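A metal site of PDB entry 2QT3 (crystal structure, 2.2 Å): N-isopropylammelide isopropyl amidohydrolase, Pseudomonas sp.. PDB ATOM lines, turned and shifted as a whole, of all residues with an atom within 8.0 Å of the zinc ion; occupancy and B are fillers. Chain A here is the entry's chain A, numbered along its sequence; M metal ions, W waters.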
ATOM      1  N   HIS A  60     -14.670   8.308 -10.962  1.00  0.00           N
ATOM      2  CA  HIS A  60     -13.841   7.228 -11.499  1.00  0.00           C
ATOM      3  C   HIS A  60     -12.533   7.123 -10.708  1.00  0.00           C
ATOM      4  O   HIS A  60     -11.621   7.947 -10.876  1.00  0.00           O
ATOM      5  CB  HIS A  60     -13.567   7.503 -12.987  1.00  0.00           C
ATOM      6  CG  HIS A  60     -12.778   6.428 -13.671  1.00  0.00           C
ATOM      7  ND1 HIS A  60     -13.254   5.774 -14.791  1.00  0.00           N
ATOM      8  CD2 HIS A  60     -11.544   5.922 -13.431  1.00  0.00           C
ATOM      9  CE1 HIS A  60     -12.342   4.906 -15.205  1.00  0.00           C
ATOM     10  NE2 HIS A  60     -11.299   4.976 -14.391  1.00  0.00           N
ATOM     11  N   THR A  61     -12.440   6.116  -9.852  1.00  0.00           N
ATOM     12  CA  THR A  61     -11.246   5.896  -9.046  1.00  0.00           C
ATOM     13  C   THR A  61     -10.798   4.420  -9.049  1.00  0.00           C
ATOM     14  O   THR A  61     -11.510   3.565  -9.565  1.00  0.00           O
ATOM     15  CB  THR A  61     -11.488   6.333  -7.589  1.00  0.00           C
ATOM     16  OG1 THR A  61     -12.590   5.596  -7.045  1.00  0.00           O
ATOM     17  CG2 THR A  61     -11.809   7.814  -7.523  1.00  0.00           C
ATOM     18  N   HIS A  62      -9.623   4.159  -8.483  1.00  0.00           N
ATOM     19  CA  HIS A  62      -9.072   2.808  -8.384  1.00  0.00           C
ATOM     20  C   HIS A  62      -8.556   2.721  -6.947  1.00  0.00           C
ATOM     21  O   HIS A  62      -7.346   2.621  -6.710  1.00  0.00           O
ATOM     22  CB  HIS A  62      -7.879   2.614  -9.349  1.00  0.00           C
ATOM     23  CG  HIS A  62      -8.279   2.550 -10.792  1.00  0.00           C
ATOM     24  ND1 HIS A  62      -8.767   1.407 -11.384  1.00  0.00           N
ATOM     25  CD2 HIS A  62      -8.299   3.506 -11.756  1.00  0.00           C
ATOM     26  CE1 HIS A  62      -9.084   1.658 -12.647  1.00  0.00           C
ATOM     27  NE2 HIS A  62      -8.807   2.922 -12.896  1.00  0.00           N
ATOM     28  N   LYS A  65      -5.768  -0.054  -5.540  1.00  0.00           N
ATOM     29  CA  LYS A  65      -4.330   0.007  -5.797  1.00  0.00           C
ATOM     30  C   LYS A  65      -3.717   1.377  -5.456  1.00  0.00           C
ATOM     31  O   LYS A  65      -2.541   1.610  -5.713  1.00  0.00           O
ATOM     32  CB  LYS A  65      -4.067  -0.315  -7.271  1.00  0.00           C
ATOM     33  CG  LYS A  65      -4.702   0.703  -8.218  1.00  0.00           C
ATOM     34  CD  LYS A  65      -4.360   0.438  -9.676  1.00  0.00           C
ATOM     35  CE  LYS A  65      -5.148  -0.734 -10.222  1.00  0.00           C
ATOM     36  NZ  LYS A  65      -5.217  -0.679 -11.702  1.00  0.00           N
ATOM     37  N   ARG A 123     -17.137   6.459  -7.570  1.00  0.00           N
ATOM     38  CA  ARG A 123     -17.280   5.178  -8.261  1.00  0.00           C
ATOM     39  C   ARG A 123     -15.874   4.615  -8.497  1.00  0.00           C
ATOM     40  O   ARG A 123     -15.101   5.177  -9.290  1.00  0.00           O
ATOM     41  CB  ARG A 123     -17.999   5.343  -9.604  1.00  0.00           C
ATOM     42  CG  ARG A 123     -18.043   4.052 -10.420  1.00  0.00           C
ATOM     43  CD  ARG A 123     -18.744   4.241 -11.758  1.00  0.00           C
ATOM     44  NE  ARG A 123     -20.177   4.470 -11.609  1.00  0.00           N
ATOM     45  CZ  ARG A 123     -20.976   4.879 -12.595  1.00  0.00           C
ATOM     46  NH1 ARG A 123     -20.466   5.109 -13.799  1.00  0.00           N
ATOM     47  NH2 ARG A 123     -22.268   5.073 -12.383  1.00  0.00           N
ATOM     48  N   THR A 124     -15.545   3.519  -7.828  1.00  0.00           N
ATOM     49  CA  THR A 124     -14.237   2.913  -7.980  1.00  0.00           C
ATOM     50  C   THR A 124     -14.297   1.650  -8.840  1.00  0.00           C
ATOM     51  O   THR A 124     -15.302   0.928  -8.838  1.00  0.00           O
ATOM     52  CB  THR A 124     -13.607   2.567  -6.586  1.00  0.00           C
ATOM     53  OG1 THR A 124     -12.230   2.222  -6.747  1.00  0.00           O
ATOM     54  CG2 THR A 124     -14.321   1.378  -5.937  1.00  0.00           C
ATOM     55  N   HIS A 125     -13.225   1.384  -9.582  1.00  0.00           N
ATOM     56  CA  HIS A 125     -13.125   0.192 -10.407  1.00  0.00           C
ATOM     57  C   HIS A 125     -12.201  -0.770  -9.674  1.00  0.00           C
ATOM     58  O   HIS A 125     -11.183  -0.347  -9.124  1.00  0.00           O
ATOM     59  CB  HIS A 125     -12.533   0.544 -11.777  1.00  0.00           C
ATOM     60  CG  HIS A 125     -13.450   1.350 -12.645  1.00  0.00           C
ATOM     61  ND1 HIS A 125     -13.738   2.675 -12.381  1.00  0.00           N
ATOM     62  CD2 HIS A 125     -14.186   1.015 -13.725  1.00  0.00           C
ATOM     63  CE1 HIS A 125     -14.615   3.113 -13.260  1.00  0.00           C
ATOM     64  NE2 HIS A 125     -14.912   2.124 -14.086  1.00  0.00           N
ATOM     65  N   ASP A 127      -9.865  -4.213  -9.966  1.00  0.00           N
ATOM     66  CA  ASP A 127      -9.221  -5.149 -10.887  1.00  0.00           C
ATOM     67  C   ASP A 127      -9.692  -6.588 -10.671  1.00  0.00           C
ATOM     68  O   ASP A 127      -9.643  -7.116  -9.565  1.00  0.00           O
ATOM     69  CB  ASP A 127      -7.694  -5.066 -10.749  1.00  0.00           C
ATOM     70  CG  ASP A 127      -7.092  -3.917 -11.563  1.00  0.00           C
ATOM     71  OD1 ASP A 127      -7.707  -2.828 -11.646  1.00  0.00           O
ATOM     72  OD2 ASP A 127      -5.982  -4.084 -12.109  1.00  0.00           O
ATOM     73  N   PHE A 158     -14.196  -4.632 -12.713  1.00  0.00           N
ATOM     74  CA  PHE A 158     -13.399  -4.260 -13.875  1.00  0.00           C
ATOM     75  C   PHE A 158     -12.530  -5.382 -14.459  1.00  0.00           C
ATOM     76  O   PHE A 158     -11.566  -5.814 -13.830  1.00  0.00           O
ATOM     77  CB  PHE A 158     -12.527  -3.044 -13.474  1.00  0.00           C
ATOM     78  CG  PHE A 158     -11.649  -2.500 -14.574  1.00  0.00           C
ATOM     79  CD1 PHE A 158     -12.120  -2.372 -15.870  1.00  0.00           C
ATOM     80  CD2 PHE A 158     -10.363  -2.038 -14.275  1.00  0.00           C
ATOM     81  CE1 PHE A 158     -11.327  -1.811 -16.861  1.00  0.00           C
ATOM     82  CE2 PHE A 158      -9.557  -1.474 -15.261  1.00  0.00           C
ATOM     83  CZ  PHE A 158     -10.048  -1.361 -16.561  1.00  0.00           C
ATOM     84  N   ASP A 215     -19.862   0.522 -17.036  1.00  0.00           N
ATOM     85  CA  ASP A 215     -18.908   1.626 -17.098  1.00  0.00           C
ATOM     86  C   ASP A 215     -17.673   1.061 -17.799  1.00  0.00           C
ATOM     87  O   ASP A 215     -16.916   0.285 -17.208  1.00  0.00           O
ATOM     88  CB  ASP A 215     -18.528   2.138 -15.697  1.00  0.00           C
ATOM     89  CG  ASP A 215     -17.714   3.420 -15.760  1.00  0.00           C
ATOM     90  OD1 ASP A 215     -16.734   3.489 -16.536  1.00  0.00           O
ATOM     91  OD2 ASP A 215     -18.045   4.379 -15.025  1.00  0.00           O
ATOM     92  N   HIS A 217     -13.969   1.240 -19.842  1.00  0.00           N
ATOM     93  CA  HIS A 217     -12.702   1.961 -19.977  1.00  0.00           C
ATOM     94  C   HIS A 217     -12.376   1.974 -21.468  1.00  0.00           C
ATOM     95  O   HIS A 217     -12.090   0.913 -22.041  1.00  0.00           O
ATOM     96  CB  HIS A 217     -11.539   1.245 -19.289  1.00  0.00           C
ATOM     97  CG  HIS A 217     -11.330   1.625 -17.859  1.00  0.00           C
ATOM     98  ND1 HIS A 217     -12.219   1.292 -16.860  1.00  0.00           N
ATOM     99  CD2 HIS A 217     -10.285   2.218 -17.243  1.00  0.00           C
ATOM    100  CE1 HIS A 217     -11.728   1.663 -15.685  1.00  0.00           C
ATOM    101  NE2 HIS A 217     -10.548   2.221 -15.890  1.00  0.00           N
ATOM    102  N   HIS A 219      -9.737   3.772 -23.782  1.00  0.00           N
ATOM    103  CA  HIS A 219      -8.553   4.603 -23.975  1.00  0.00           C
ATOM    104  C   HIS A 219      -8.130   4.787 -25.422  1.00  0.00           C
ATOM    105  O   HIS A 219      -7.467   5.758 -25.744  1.00  0.00           O
ATOM    106  CB  HIS A 219      -7.323   4.015 -23.267  1.00  0.00           C
ATOM    107  CG  HIS A 219      -7.506   3.778 -21.805  1.00  0.00           C
ATOM    108  ND1 HIS A 219      -7.896   2.562 -21.297  1.00  0.00           N
ATOM    109  CD2 HIS A 219      -7.309   4.590 -20.735  1.00  0.00           C
ATOM    110  CE1 HIS A 219      -7.921   2.619 -19.980  1.00  0.00           C
ATOM    111  NE2 HIS A 219      -7.566   3.839 -19.617  1.00  0.00           N
ATOM    112  N   SER A 248     -15.677   5.728 -19.813  1.00  0.00           N
ATOM    113  CA  SER A 248     -14.644   6.475 -19.104  1.00  0.00           C
ATOM    114  C   SER A 248     -13.478   6.872 -20.012  1.00  0.00           C
ATOM    115  O   SER A 248     -13.071   6.100 -20.879  1.00  0.00           O
ATOM    116  CB  SER A 248     -14.121   5.657 -17.912  1.00  0.00           C
ATOM    117  OG  SER A 248     -15.085   5.610 -16.862  1.00  0.00           O
ATOM    118  N   HIS A 249     -12.977   8.092 -19.816  1.00  0.00           N
ATOM    119  CA  HIS A 249     -11.864   8.663 -20.577  1.00  0.00           C
ATOM    120  C   HIS A 249     -12.231   9.260 -21.926  1.00  0.00           C
ATOM    121  O   HIS A 249     -12.239  10.478 -22.083  1.00  0.00           O
ATOM    122  CB  HIS A 249     -10.739   7.643 -20.766  1.00  0.00           C
ATOM    123  CG  HIS A 249     -10.108   7.206 -19.473  1.00  0.00           C
ATOM    124  ND1 HIS A 249      -9.661   8.097 -18.530  1.00  0.00           N
ATOM    125  CD2 HIS A 249      -9.859   5.963 -18.976  1.00  0.00           C
ATOM    126  CE1 HIS A 249      -9.163   7.426 -17.495  1.00  0.00           C
ATOM    127  NE2 HIS A 249      -9.268   6.134 -17.750  1.00  0.00           N
ATOM    128  N   CYS A 278     -11.066  12.161 -16.622  1.00  0.00           N
ATOM    129  CA  CYS A 278     -10.275  12.250 -15.389  1.00  0.00           C
ATOM    130  C   CYS A 278      -9.257  13.389 -15.488  1.00  0.00           C
ATOM    131  O   CYS A 278      -8.513  13.471 -16.464  1.00  0.00           O
ATOM    132  CB  CYS A 278      -9.572  10.909 -15.137  1.00  0.00           C
ATOM    133  SG  CYS A 278     -10.747   9.504 -15.002  1.00  0.00           S
ATOM    134  N   SER A 302     -10.647  11.657 -10.348  1.00  0.00           N
ATOM    135  CA  SER A 302      -9.227  11.593 -10.014  1.00  0.00           C
ATOM    136  C   SER A 302      -8.499  10.499 -10.805  1.00  0.00           C
ATOM    137  O   SER A 302      -7.340  10.662 -11.186  1.00  0.00           O
ATOM    138  CB  SER A 302      -9.035  11.249  -8.528  1.00  0.00           C
ATOM    139  OG  SER A 302      -9.538  12.250  -7.653  1.00  0.00           O
ATOM    140  N   ASP A 303      -9.225   9.408 -11.058  1.00  0.00           N
ATOM    141  CA  ASP A 303      -8.667   8.207 -11.663  1.00  0.00           C
ATOM    142  C   ASP A 303      -7.637   7.787 -10.619  1.00  0.00           C
ATOM    143  O   ASP A 303      -7.796   8.109  -9.438  1.00  0.00           O
ATOM    144  CB  ASP A 303      -7.978   8.462 -13.013  1.00  0.00           C
ATOM    145  CG  ASP A 303      -7.912   7.187 -13.877  1.00  0.00           C
ATOM    146  OD1 ASP A 303      -8.459   6.134 -13.453  1.00  0.00           O
ATOM    147  OD2 ASP A 303      -7.337   7.232 -14.991  1.00  0.00           O
ATOM    148  N   ASN A 304      -6.585   7.101 -11.041  1.00  0.00           N
ATOM    149  CA  ASN A 304      -5.564   6.624 -10.122  1.00  0.00           C
ATOM    150  C   ASN A 304      -4.977   7.679  -9.200  1.00  0.00           C
ATOM    151  O   ASN A 304      -4.830   8.847  -9.568  1.00  0.00           O
ATOM    152  CB  ASN A 304      -4.434   5.983 -10.917  1.00  0.00           C
ATOM    153  CG  ASN A 304      -4.913   4.836 -11.790  1.00  0.00           C
ATOM    154  OD1 ASN A 304      -4.694   3.676 -11.490  1.00  0.00           O
ATOM    155  ND2 ASN A 304      -5.574   5.176 -12.882  1.00  0.00           N
ATOM    156  N   TRP A 309       0.328   3.943 -12.045  1.00  0.00           N
ATOM    157  CA  TRP A 309      -0.289   4.503 -13.261  1.00  0.00           C
ATOM    158  C   TRP A 309      -0.249   6.022 -13.223  1.00  0.00           C
ATOM    159  O   TRP A 309      -0.040   6.665 -14.244  1.00  0.00           O
ATOM    160  CB  TRP A 309      -1.740   4.049 -13.405  1.00  0.00           C
ATOM    161  CG  TRP A 309      -1.878   2.628 -13.818  1.00  0.00           C
ATOM    162  CD1 TRP A 309      -2.304   1.574 -13.050  1.00  0.00           C
ATOM    163  CD2 TRP A 309      -1.534   2.077 -15.092  1.00  0.00           C
ATOM    164  NE1 TRP A 309      -2.250   0.410 -13.773  1.00  0.00           N
ATOM    165  CE2 TRP A 309      -1.779   0.686 -15.030  1.00  0.00           C
ATOM    166  CE3 TRP A 309      -1.044   2.625 -16.278  1.00  0.00           C
ATOM    167  CZ2 TRP A 309      -1.551  -0.161 -16.113  1.00  0.00           C
ATOM    168  CZ3 TRP A 309      -0.807   1.781 -17.365  1.00  0.00           C
ATOM    169  CH2 TRP A 309      -1.062   0.400 -17.263  1.00  0.00           C
HETATM  170 ZN    ZN M   1      -9.514   3.885 -14.605  1.00  0.00          ZN
HETATM  171  O   HOH W   1      -7.884   4.441 -15.851  1.00  0.00           O
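Water W1 bridges NE2 of His 249 and OD2 of Asp 303.
Merely in contact with the zinc ion: His 249. Of the 19 residues printed, 5 come within 4 Å of the zinc ion. The nearest printed residue that does not touch the zinc ion is Asn 304 (4.5 Å).
OD1 of Asp 303 sits close to NE2 of His 62, 3.3 Å away. The backbone carbonyl oxygen (O) of His 60 lies within hydrogen-bond range of the backbone NH (N) of Asp 303 (2.8 Å). The side-chain hydroxyl (OG) of Ser 248 lies within hydrogen-bond range of a ring nitrogen (ND1) of His 60, at 2.8 Å. The side-chain amide nitrogen (ND2) of Asn 304 lies within hydrogen-bond range of the side-chain carboxylate (OD1) of Asp 303 (3.1 Å). NE2 of His 249 lies close to NE2 of His 219 (3.4 Å).
The zinc ion is bound by NE2 of His 62, NE2 of His 60, water W1 and NE2 of His 217. The zinc ion has four donor atoms within binding distance. Slightly farther from the zinc ion lies OD1 of Asp 303 (2.7 Å).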
